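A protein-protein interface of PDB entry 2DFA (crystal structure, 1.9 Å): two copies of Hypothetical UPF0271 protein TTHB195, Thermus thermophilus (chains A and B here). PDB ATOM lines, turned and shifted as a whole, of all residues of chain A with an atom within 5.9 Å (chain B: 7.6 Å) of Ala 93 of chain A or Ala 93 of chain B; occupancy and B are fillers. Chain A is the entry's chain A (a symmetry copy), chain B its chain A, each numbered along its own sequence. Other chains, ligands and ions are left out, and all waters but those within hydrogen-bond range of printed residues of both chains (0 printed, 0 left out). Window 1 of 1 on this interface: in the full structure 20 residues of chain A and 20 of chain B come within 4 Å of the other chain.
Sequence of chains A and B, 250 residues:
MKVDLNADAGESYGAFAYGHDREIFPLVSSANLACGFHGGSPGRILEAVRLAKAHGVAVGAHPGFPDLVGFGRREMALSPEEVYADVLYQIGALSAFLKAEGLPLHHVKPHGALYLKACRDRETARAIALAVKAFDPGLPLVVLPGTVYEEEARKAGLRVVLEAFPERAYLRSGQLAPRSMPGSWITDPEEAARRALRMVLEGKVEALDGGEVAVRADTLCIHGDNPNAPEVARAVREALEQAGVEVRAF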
ATOM      1  N   CYS A  35     -21.425  12.142 -13.357  1.00  0.00           N
ATOM      2  CA  CYS A  35     -21.794  11.647 -14.676  1.00  0.00           C
ATOM      3  C   CYS A  35     -20.960  10.499 -15.249  1.00  0.00           C
ATOM      4  O   CYS A  35     -20.862  10.361 -16.471  1.00  0.00           O
ATOM      5  CB  CYS A  35     -21.801  12.825 -15.659  1.00  0.00           C
ATOM      6  SG  CYS A  35     -22.781  14.262 -15.081  1.00  0.00           S
ATOM      7  N   ILE A  45     -26.419   6.362 -11.257  1.00  0.00           N
ATOM      8  CA  ILE A  45     -26.987   7.628 -11.703  1.00  0.00           C
ATOM      9  C   ILE A  45     -28.504   7.478 -11.686  1.00  0.00           C
ATOM     10  O   ILE A  45     -29.222   8.325 -11.147  1.00  0.00           O
ATOM     11  CB  ILE A  45     -26.525   7.986 -13.140  1.00  0.00           C
ATOM     12  CG1 ILE A  45     -25.025   8.314 -13.136  1.00  0.00           C
ATOM     13  CG2 ILE A  45     -27.336   9.165 -13.675  1.00  0.00           C
ATOM     14  CD1 ILE A  45     -24.452   8.643 -14.515  1.00  0.00           C
ATOM     15  N   LEU A  88     -19.622  17.915 -22.479  1.00  0.00           N
ATOM     16  CA  LEU A  88     -20.811  17.635 -23.290  1.00  0.00           C
ATOM     17  C   LEU A  88     -21.269  16.193 -23.098  1.00  0.00           C
ATOM     18  O   LEU A  88     -22.455  15.915 -22.910  1.00  0.00           O
ATOM     19  CB  LEU A  88     -20.522  17.840 -24.778  1.00  0.00           C
ATOM     20  CG  LEU A  88     -20.921  19.163 -25.419  1.00  0.00           C
ATOM     21  CD1 LEU A  88     -20.603  19.114 -26.910  1.00  0.00           C
ATOM     22  CD2 LEU A  88     -22.410  19.405 -25.209  1.00  0.00           C
ATOM     23  N   TYR A  89     -20.308  15.277 -23.177  1.00  0.00           N
ATOM     24  CA  TYR A  89     -20.567  13.856 -23.023  1.00  0.00           C
ATOM     25  C   TYR A  89     -21.279  13.577 -21.703  1.00  0.00           C
ATOM     26  O   TYR A  89     -22.273  12.859 -21.660  1.00  0.00           O
ATOM     27  CB  TYR A  89     -19.230  13.092 -23.063  1.00  0.00           C
ATOM     28  CG  TYR A  89     -19.349  11.588 -22.980  1.00  0.00           C
ATOM     29  CD1 TYR A  89     -19.619  10.947 -21.762  1.00  0.00           C
ATOM     30  CD2 TYR A  89     -19.196  10.799 -24.121  1.00  0.00           C
ATOM     31  CE1 TYR A  89     -19.731   9.564 -21.685  1.00  0.00           C
ATOM     32  CE2 TYR A  89     -19.311   9.413 -24.058  1.00  0.00           C
ATOM     33  CZ  TYR A  89     -19.579   8.800 -22.840  1.00  0.00           C
ATOM     34  OH  TYR A  89     -19.711   7.436 -22.779  1.00  0.00           O
ATOM     35  N   GLN A  90     -20.752  14.148 -20.627  1.00  0.00           N
ATOM     36  CA  GLN A  90     -21.311  13.934 -19.297  1.00  0.00           C
ATOM     37  C   GLN A  90     -22.695  14.534 -19.113  1.00  0.00           C
ATOM     38  O   GLN A  90     -23.591  13.887 -18.575  1.00  0.00           O
ATOM     39  CB  GLN A  90     -20.345  14.479 -18.251  1.00  0.00           C
ATOM     40  CG  GLN A  90     -19.056  13.648 -18.161  1.00  0.00           C
ATOM     41  CD  GLN A  90     -18.063  14.202 -17.167  1.00  0.00           C
ATOM     42  OE1 GLN A  90     -18.189  13.987 -15.959  1.00  0.00           O
ATOM     43  NE2 GLN A  90     -17.064  14.921 -17.666  1.00  0.00           N
ATOM     44  N   ILE A  91     -22.868  15.773 -19.555  1.00  0.00           N
ATOM     45  CA  ILE A  91     -24.172  16.426 -19.437  1.00  0.00           C
ATOM     46  C   ILE A  91     -25.201  15.607 -20.202  1.00  0.00           C
ATOM     47  O   ILE A  91     -26.311  15.382 -19.725  1.00  0.00           O
ATOM     48  CB  ILE A  91     -24.138  17.858 -20.020  1.00  0.00           C
ATOM     49  CG1 ILE A  91     -23.325  18.769 -19.100  1.00  0.00           C
ATOM     50  CG2 ILE A  91     -25.564  18.385 -20.203  1.00  0.00           C
ATOM     51  CD1 ILE A  91     -23.109  20.165 -19.674  1.00  0.00           C
ATOM     52  N   GLY A  92     -24.830  15.163 -21.398  1.00  0.00           N
ATOM     53  CA  GLY A  92     -25.751  14.371 -22.197  1.00  0.00           C
ATOM     54  C   GLY A  92     -26.154  13.066 -21.541  1.00  0.00           C
ATOM     55  O   GLY A  92     -27.340  12.707 -21.531  1.00  0.00           O
ATOM     56  N   ALA A  93     -25.173  12.351 -20.990  1.00  0.00           N
ATOM     57  CA  ALA A  93     -25.452  11.075 -20.342  1.00  0.00           C
ATOM     58  C   ALA A  93     -26.458  11.248 -19.206  1.00  0.00           C
ATOM     59  O   ALA A  93     -27.417  10.492 -19.111  1.00  0.00           O
ATOM     60  CB  ALA A  93     -24.159  10.448 -19.812  1.00  0.00           C
ATOM     61  N   LEU A  94     -26.232  12.237 -18.345  1.00  0.00           N
ATOM     62  CA  LEU A  94     -27.141  12.479 -17.229  1.00  0.00           C
ATOM     63  C   LEU A  94     -28.529  12.880 -17.726  1.00  0.00           C
ATOM     64  O   LEU A  94     -29.545  12.410 -17.199  1.00  0.00           O
ATOM     65  CB  LEU A  94     -26.582  13.571 -16.302  1.00  0.00           C
ATOM     66  CG  LEU A  94     -27.519  13.995 -15.160  1.00  0.00           C
ATOM     67  CD1 LEU A  94     -27.834  12.804 -14.269  1.00  0.00           C
ATOM     68  CD2 LEU A  94     -26.877  15.112 -14.354  1.00  0.00           C
ATOM     69  N   SER A  95     -28.576  13.718 -18.760  1.00  0.00           N
ATOM     70  CA  SER A  95     -29.862  14.171 -19.295  1.00  0.00           C
ATOM     71  C   SER A  95     -30.763  13.037 -19.766  1.00  0.00           C
ATOM     72  O   SER A  95     -31.983  13.182 -19.762  1.00  0.00           O
ATOM     73  CB  SER A  95     -29.658  15.167 -20.441  1.00  0.00           C
ATOM     74  OG  SER A  95     -29.221  14.509 -21.620  1.00  0.00           O
ATOM     75  N   ALA A  96     -30.175  11.911 -20.169  1.00  0.00           N
ATOM     76  CA  ALA A  96     -30.970  10.775 -20.623  1.00  0.00           C
ATOM     77  C   ALA A  96     -31.774  10.189 -19.460  1.00  0.00           C
ATOM     78  O   ALA A  96     -32.930   9.813 -19.632  1.00  0.00           O
ATOM     79  CB  ALA A  96     -30.071   9.696 -21.242  1.00  0.00           C
ATOM     80  N   PHE A  97     -31.159  10.108 -18.282  1.00  0.00           N
ATOM     81  CA  PHE A  97     -31.839   9.586 -17.099  1.00  0.00           C
ATOM     82  C   PHE A  97     -32.941  10.544 -16.643  1.00  0.00           C
ATOM     83  O   PHE A  97     -34.005  10.116 -16.197  1.00  0.00           O
ATOM     84  CB  PHE A  97     -30.831   9.366 -15.972  1.00  0.00           C
ATOM     85  CG  PHE A  97     -29.889   8.234 -16.237  1.00  0.00           C
ATOM     86  CD1 PHE A  97     -30.286   6.919 -16.024  1.00  0.00           C
ATOM     87  CD2 PHE A  97     -28.628   8.473 -16.769  1.00  0.00           C
ATOM     88  CE1 PHE A  97     -29.438   5.855 -16.346  1.00  0.00           C
ATOM     89  CE2 PHE A  97     -27.780   7.416 -17.091  1.00  0.00           C
ATOM     90  CZ  PHE A  97     -28.186   6.111 -16.879  1.00  0.00           C
ATOM     91  N   ALA B  34     -20.238   4.909 -31.943  1.00  0.00           N
ATOM     92  CA  ALA B  34     -19.939   4.339 -30.635  1.00  0.00           C
ATOM     93  C   ALA B  34     -20.187   5.417 -29.582  1.00  0.00           C
ATOM     94  O   ALA B  34     -20.074   6.616 -29.866  1.00  0.00           O
ATOM     95  CB  ALA B  34     -18.478   3.862 -30.581  1.00  0.00           C
ATOM     96  N   CYS B  35     -20.504   4.992 -28.359  1.00  0.00           N
ATOM     97  CA  CYS B  35     -20.813   5.940 -27.298  1.00  0.00           C
ATOM     98  C   CYS B  35     -19.908   5.926 -26.064  1.00  0.00           C
ATOM     99  O   CYS B  35     -20.350   6.294 -24.973  1.00  0.00           O
ATOM    100  CB  CYS B  35     -22.274   5.742 -26.872  1.00  0.00           C
ATOM    101  SG  CYS B  35     -23.458   5.750 -28.271  1.00  0.00           S
ATOM    102  N   GLY B  36     -18.656   5.501 -26.230  1.00  0.00           N
ATOM    103  CA  GLY B  36     -17.715   5.506 -25.120  1.00  0.00           C
ATOM    104  C   GLY B  36     -17.547   4.242 -24.292  1.00  0.00           C
ATOM    105  O   GLY B  36     -16.695   4.208 -23.401  1.00  0.00           O
ATOM    106  N   PHE B  37     -18.330   3.207 -24.572  1.00  0.00           N
ATOM    107  CA  PHE B  37     -18.227   1.958 -23.808  1.00  0.00           C
ATOM    108  C   PHE B  37     -17.322   0.908 -24.453  1.00  0.00           C
ATOM    109  O   PHE B  37     -16.472   0.319 -23.777  1.00  0.00           O
ATOM    110  CB  PHE B  37     -19.621   1.358 -23.583  1.00  0.00           C
ATOM    111  CG  PHE B  37     -20.358   1.943 -22.404  1.00  0.00           C
ATOM    112  CD1 PHE B  37     -20.339   3.311 -22.155  1.00  0.00           C
ATOM    113  CD2 PHE B  37     -21.095   1.117 -21.554  1.00  0.00           C
ATOM    114  CE1 PHE B  37     -21.045   3.855 -21.073  1.00  0.00           C
ATOM    115  CE2 PHE B  37     -21.807   1.646 -20.467  1.00  0.00           C
ATOM    116  CZ  PHE B  37     -21.781   3.011 -20.227  1.00  0.00           C
ATOM    117  N   PRO B  42     -14.894  10.722 -25.933  1.00  0.00           N
ATOM    118  CA  PRO B  42     -15.580  11.990 -26.229  1.00  0.00           C
ATOM    119  C   PRO B  42     -15.073  12.792 -27.433  1.00  0.00           C
ATOM    120  O   PRO B  42     -15.867  13.229 -28.274  1.00  0.00           O
ATOM    121  CB  PRO B  42     -15.459  12.768 -24.921  1.00  0.00           C
ATOM    122  CG  PRO B  42     -15.494  11.664 -23.878  1.00  0.00           C
ATOM    123  CD  PRO B  42     -14.575  10.618 -24.494  1.00  0.00           C
ATOM    124  N   ILE B  45     -15.933  11.054 -30.620  1.00  0.00           N
ATOM    125  CA  ILE B  45     -17.356  11.118 -30.929  1.00  0.00           C
ATOM    126  C   ILE B  45     -17.612  12.452 -31.620  1.00  0.00           C
ATOM    127  O   ILE B  45     -18.251  12.512 -32.674  1.00  0.00           O
ATOM    128  CB  ILE B  45     -18.224  11.031 -29.647  1.00  0.00           C
ATOM    129  CG1 ILE B  45     -18.110   9.626 -29.038  1.00  0.00           C
ATOM    130  CG2 ILE B  45     -19.679  11.365 -29.972  1.00  0.00           C
ATOM    131  CD1 ILE B  45     -18.898   9.440 -27.740  1.00  0.00           C
ATOM    132  N   ALA B  85     -29.905   0.914 -18.085  1.00  0.00           N
ATOM    133  CA  ALA B  85     -29.141   2.073 -17.638  1.00  0.00           C
ATOM    134  C   ALA B  85     -27.954   2.377 -18.553  1.00  0.00           C
ATOM    135  O   ALA B  85     -27.692   3.535 -18.882  1.00  0.00           O
ATOM    136  CB  ALA B  85     -28.645   1.855 -16.196  1.00  0.00           C
ATOM    137  N   VAL B  87     -27.576   1.584 -21.753  1.00  0.00           N
ATOM    138  CA  VAL B  87     -28.056   2.072 -23.045  1.00  0.00           C
ATOM    139  C   VAL B  87     -28.512   3.524 -22.934  1.00  0.00           C
ATOM    140  O   VAL B  87     -28.204   4.347 -23.802  1.00  0.00           O
ATOM    141  CB  VAL B  87     -29.211   1.196 -23.584  1.00  0.00           C
ATOM    142  CG1 VAL B  87     -29.851   1.847 -24.826  1.00  0.00           C
ATOM    143  CG2 VAL B  87     -28.669  -0.183 -23.945  1.00  0.00           C
ATOM    144  N   LEU B  88     -29.244   3.852 -21.871  1.00  0.00           N
ATOM    145  CA  LEU B  88     -29.703   5.233 -21.686  1.00  0.00           C
ATOM    146  C   LEU B  88     -28.518   6.190 -21.602  1.00  0.00           C
ATOM    147  O   LEU B  88     -28.501   7.248 -22.234  1.00  0.00           O
ATOM    148  CB  LEU B  88     -30.512   5.375 -20.395  1.00  0.00           C
ATOM    149  CG  LEU B  88     -32.032   5.334 -20.482  1.00  0.00           C
ATOM    150  CD1 LEU B  88     -32.621   5.564 -19.095  1.00  0.00           C
ATOM    151  CD2 LEU B  88     -32.519   6.412 -21.443  1.00  0.00           C
ATOM    152  N   TYR B  89     -27.539   5.810 -20.786  1.00  0.00           N
ATOM    153  CA  TYR B  89     -26.339   6.602 -20.582  1.00  0.00           C
ATOM    154  C   TYR B  89     -25.658   6.902 -21.915  1.00  0.00           C
ATOM    155  O   TYR B  89     -25.290   8.038 -22.195  1.00  0.00           O
ATOM    156  CB  TYR B  89     -25.372   5.826 -19.668  1.00  0.00           C
ATOM    157  CG  TYR B  89     -24.099   6.560 -19.313  1.00  0.00           C
ATOM    158  CD1 TYR B  89     -23.049   6.680 -20.234  1.00  0.00           C
ATOM    159  CD2 TYR B  89     -23.942   7.142 -18.054  1.00  0.00           C
ATOM    160  CE1 TYR B  89     -21.879   7.357 -19.910  1.00  0.00           C
ATOM    161  CE2 TYR B  89     -22.777   7.827 -17.718  1.00  0.00           C
ATOM    162  CZ  TYR B  89     -21.749   7.933 -18.648  1.00  0.00           C
ATOM    163  OH  TYR B  89     -20.609   8.623 -18.326  1.00  0.00           O
ATOM    164  N   GLN B  90     -25.488   5.865 -22.726  1.00  0.00           N
ATOM    165  CA  GLN B  90     -24.816   6.004 -24.013  1.00  0.00           C
ATOM    166  C   GLN B  90     -25.589   6.844 -25.016  1.00  0.00           C
ATOM    167  O   GLN B  90     -25.020   7.709 -25.678  1.00  0.00           O
ATOM    168  CB  GLN B  90     -24.526   4.619 -24.582  1.00  0.00           C
ATOM    169  CG  GLN B  90     -23.454   3.873 -23.775  1.00  0.00           C
ATOM    170  CD  GLN B  90     -23.187   2.479 -24.291  1.00  0.00           C
ATOM    171  OE1 GLN B  90     -22.463   2.294 -25.272  1.00  0.00           O
ATOM    172  NE2 GLN B  90     -23.773   1.483 -23.635  1.00  0.00           N
ATOM    173  N   ILE B  91     -26.886   6.587 -25.133  1.00  0.00           N
ATOM    174  CA  ILE B  91     -27.714   7.358 -26.059  1.00  0.00           C
ATOM    175  C   ILE B  91     -27.657   8.826 -25.664  1.00  0.00           C
ATOM    176  O   ILE B  91     -27.525   9.705 -26.512  1.00  0.00           O
ATOM    177  CB  ILE B  91     -29.186   6.886 -26.023  1.00  0.00           C
ATOM    178  CG1 ILE B  91     -29.303   5.511 -26.679  1.00  0.00           C
ATOM    179  CG2 ILE B  91     -30.084   7.911 -26.722  1.00  0.00           C
ATOM    180  CD1 ILE B  91     -30.694   4.900 -26.551  1.00  0.00           C
ATOM    181  N   GLY B  92     -27.758   9.091 -24.366  1.00  0.00           N
ATOM    182  CA  GLY B  92     -27.713  10.467 -23.899  1.00  0.00           C
ATOM    183  C   GLY B  92     -26.407  11.169 -24.212  1.00  0.00           C
ATOM    184  O   GLY B  92     -26.406  12.320 -24.672  1.00  0.00           O
ATOM    185  N   ALA B  93     -25.290  10.483 -23.966  1.00  0.00           N
ATOM    186  CA  ALA B  93     -23.981  11.071 -24.224  1.00  0.00           C
ATOM    187  C   ALA B  93     -23.843  11.478 -25.689  1.00  0.00           C
ATOM    188  O   ALA B  93     -23.409  12.585 -25.984  1.00  0.00           O
ATOM    189  CB  ALA B  93     -22.869  10.091 -23.840  1.00  0.00           C
ATOM    190  N   LEU B  94     -24.205  10.579 -26.601  1.00  0.00           N
ATOM    191  CA  LEU B  94     -24.109  10.880 -28.026  1.00  0.00           C
ATOM    192  C   LEU B  94     -25.041  12.029 -28.410  1.00  0.00           C
ATOM    193  O   LEU B  94     -24.656  12.921 -29.176  1.00  0.00           O
ATOM    194  CB  LEU B  94     -24.439   9.636 -28.866  1.00  0.00           C
ATOM    195  CG  LEU B  94     -24.492   9.873 -30.384  1.00  0.00           C
ATOM    196  CD1 LEU B  94     -23.147  10.375 -30.884  1.00  0.00           C
ATOM    197  CD2 LEU B  94     -24.880   8.587 -31.093  1.00  0.00           C
ATOM    198  N   SER B  95     -26.250  12.030 -27.853  1.00  0.00           N
ATOM    199  CA  SER B  95     -27.218  13.082 -28.174  1.00  0.00           C
ATOM    200  C   SER B  95     -26.722  14.488 -27.857  1.00  0.00           C
ATOM    201  O   SER B  95     -27.157  15.447 -28.489  1.00  0.00           O
ATOM    202  CB  SER B  95     -28.549  12.839 -27.456  1.00  0.00           C
ATOM    203  OG  SER B  95     -28.447  13.137 -26.072  1.00  0.00           O
ATOM    204  N   ALA B  96     -25.818  14.616 -26.887  1.00  0.00           N
ATOM    205  CA  ALA B  96     -25.285  15.927 -26.533  1.00  0.00           C
ATOM    206  C   ALA B  96     -24.444  16.489 -27.681  1.00  0.00           C
ATOM    207  O   ALA B  96     -24.509  17.680 -27.973  1.00  0.00           O
ATOM    208  CB  ALA B  96     -24.443  15.843 -25.252  1.00  0.00           C
ATOM    209  N   PHE B  97     -23.656  15.632 -28.327  1.00  0.00           N
ATOM    210  CA  PHE B  97     -22.827  16.055 -29.453  1.00  0.00           C
ATOM    211  C   PHE B  97     -23.698  16.414 -30.658  1.00  0.00           C
ATOM    212  O   PHE B  97     -23.400  17.354 -31.395  1.00  0.00           O
ATOM    213  CB  PHE B  97     -21.845  14.945 -29.824  1.00  0.00           C
ATOM    214  CG  PHE B  97     -20.777  14.736 -28.797  1.00  0.00           C
ATOM    215  CD1 PHE B  97     -19.674  15.579 -28.741  1.00  0.00           C
ATOM    216  CD2 PHE B  97     -20.907  13.741 -27.835  1.00  0.00           C
ATOM    217  CE1 PHE B  97     -18.715  15.436 -27.733  1.00  0.00           C
ATOM    218  CE2 PHE B  97     -19.955  13.596 -26.829  1.00  0.00           C
ATOM    219  CZ  PHE B  97     -18.862  14.442 -26.781  1.00  0.00           C
ATOM    220  N   LEU B  98     -24.775  15.665 -30.857  1.00  0.00           N
ATOM    221  CA  LEU B  98     -25.678  15.949 -31.966  1.00  0.00           C
ATOM    222  C   LEU B  98     -26.378  17.285 -31.715  1.00  0.00           C
ATOM    223  O   LEU B  98     -26.558  18.085 -32.635  1.00  0.00           O
ATOM    224  CB  LEU B  98     -26.703  14.820 -32.111  1.00  0.00           C
ATOM    225  CG  LEU B  98     -26.073  13.468 -32.449  1.00  0.00           C
ATOM    226  CD1 LEU B  98     -27.115  12.357 -32.383  1.00  0.00           C
ATOM    227  CD2 LEU B  98     -25.445  13.551 -33.834  1.00  0.00           C
ATOM    228  N   LYS B  99     -26.764  17.526 -30.464  1.00  0.00           N
ATOM    229  CA  LYS B  99     -27.424  18.773 -30.100  1.00  0.00           C
ATOM    230  C   LYS B  99     -26.498  19.959 -30.363  1.00  0.00           C
ATOM    231  O   LYS B  99     -26.928  20.979 -30.910  1.00  0.00           O
ATOM    232  CB  LYS B  99     -27.844  18.742 -28.621  1.00  0.00           C
ATOM    233  CG  LYS B  99     -28.300  20.082 -28.056  1.00  0.00           C
ATOM    234  CD  LYS B  99     -29.589  20.595 -28.702  1.00  0.00           C
ATOM    235  CE  LYS B  99     -29.937  21.985 -28.166  1.00  0.00           C
ATOM    236  NZ  LYS B  99     -31.148  22.566 -28.816  1.00  0.00           N
ATOM    237  N   PHE B 135     -36.174   7.431 -23.706  1.00  0.00           N
ATOM    238  CA  PHE B 135     -35.430   8.605 -24.159  1.00  0.00           C
ATOM    239  C   PHE B 135     -36.207   9.403 -25.209  1.00  0.00           C
ATOM    240  O   PHE B 135     -36.274  10.626 -25.138  1.00  0.00           O
ATOM    241  CB  PHE B 135     -34.085   8.186 -24.759  1.00  0.00           C
ATOM    242  CG  PHE B 135     -33.207   9.344 -25.147  1.00  0.00           C
ATOM    243  CD1 PHE B 135     -32.531  10.080 -24.174  1.00  0.00           C
ATOM    244  CD2 PHE B 135     -33.067   9.713 -26.480  1.00  0.00           C
ATOM    245  CE1 PHE B 135     -31.731  11.166 -24.528  1.00  0.00           C
ATOM    246  CE2 PHE B 135     -32.267  10.798 -26.840  1.00  0.00           C
ATOM    247  CZ  PHE B 135     -31.601  11.524 -25.862  1.00  0.00           C
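OH of Tyr 89 of chain A lies within hydrogen-bond range of O of Cys 35 of chain B, 2.6 Å away.
The backbone carbonyl oxygen (O) of Gly 92 of chain A lies close to the backbone carbonyl oxygen (O) of Gly 92 of chain B.
O of Cys 35 of chain A sits at hydrogen-bond distance from OH of Tyr 89 of chain B (2.6 Å).
SG of Cys 35 of chain B sits close to O of Gln 90 of chain B (3.6 Å).
O of Gln 90 of chain A lies close to SG of Cys 35 of chain A (3.6 Å).
O of Gly 92 of chain A lies within hydrogen-bond range of OG of Ser 95 of chain A (2.6 Å).
The backbone carbonyl oxygen (O) of Gly 92 of chain B lies within hydrogen-bond range of the side-chain hydroxyl (OG) of Ser 95 of chain B (2.6 Å).
Tyr 89 of chain A touches Pro 42 of chain B.
CE2 of Tyr 89 of chain A touches CD1 of Ile 45 of chain B (3.7 Å).
CE1 of Tyr 89 of chain A touches CE1 of Tyr 89 of chain B, 3.6 Å away.
CE2 of Phe 97 of chain B touches CA of Tyr 89 of chain A, 3.9 Å away.
C of Gly 92 of chain A touches N of Ala 93 of chain B, 3.6 Å away.
Ala 93 of chain A touches Tyr 89 of chain B.
Leu 88 of chain B touches Ala 96 of chain A (O to CB, 3.1 Å).
CB of Ala 96 of chain A touches CD1 of Phe 135 of chain B, 3.8 Å away.
Phe 97 of chain A touches Ala 85 of chain B (CZ to O, 3.3 Å).
Phe 97 of chain A touches Tyr 89 of chain B.
Of chain B, only Tyr 89 (3.6 Å), Gly 92 (3.6 Å) and Ala 93 (3.5 Å) come within 4 Å of Ala 93 of chain A.
Gly 92 of chain A touches just these residues of chain B: Gly 92 (3.2 Å), Ala 93 (3.6 Å) and Ala 96 (3.6 Å).
Of the printed residues of chain A, Cys 35 of chain B touches Tyr 89.
Printed residues of chain B within 4 Å of Leu 88 of chain A: Ala 96.
Printed residues of chain A within 4 Å of Ala 85 of chain B: Phe 97.
Val 87 of chain B touches none of the printed residues of chain A.
Phe 37 of chain B touches none of the printed residues of chain A.
The nearest residue of chain B that does not touch Ala 93 of chain A is Leu 88 of chain B (4.6 Å).
The nearest residue of chain A that does not touch Ala 93 of chain B is Leu 88 of chain A (4.6 Å).
The nearest printed residue of chain A that does not touch Phe 97 of chain B is Leu 88 of chain A (4.1 Å).
Hydrophobic or aromatic side chains of chain B that line the printed part of chain A: Pro 42, Ile 45, Leu 88, Tyr 89, Ala 93, Ala 96, Phe 97 and Phe 135.
Along chain B the printed residues that touch a printed residue of chain A span positions 35 to 135.
Among the printed residues, 21 pairs touch across the chains.
Cys 35 of chain A touches Tyr 89 of chain B, and with the chains exchanged Tyr 89 of chain A touches Cys 35 of chain B.
Tyr 89 of chain A touches Phe 97 of chain B, and with the chains exchanged Phe 97 of chain A touches Tyr 89 of chain B.
Gly 92 of chain B touches its own counterpart, Gly 92 of chain A.
Gly 92 of chain A touches Ala 96 of chain B, and with the chains exchanged Ala 96 of chain A touches Gly 92 of chain B.
12 positions are printed for both chains.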
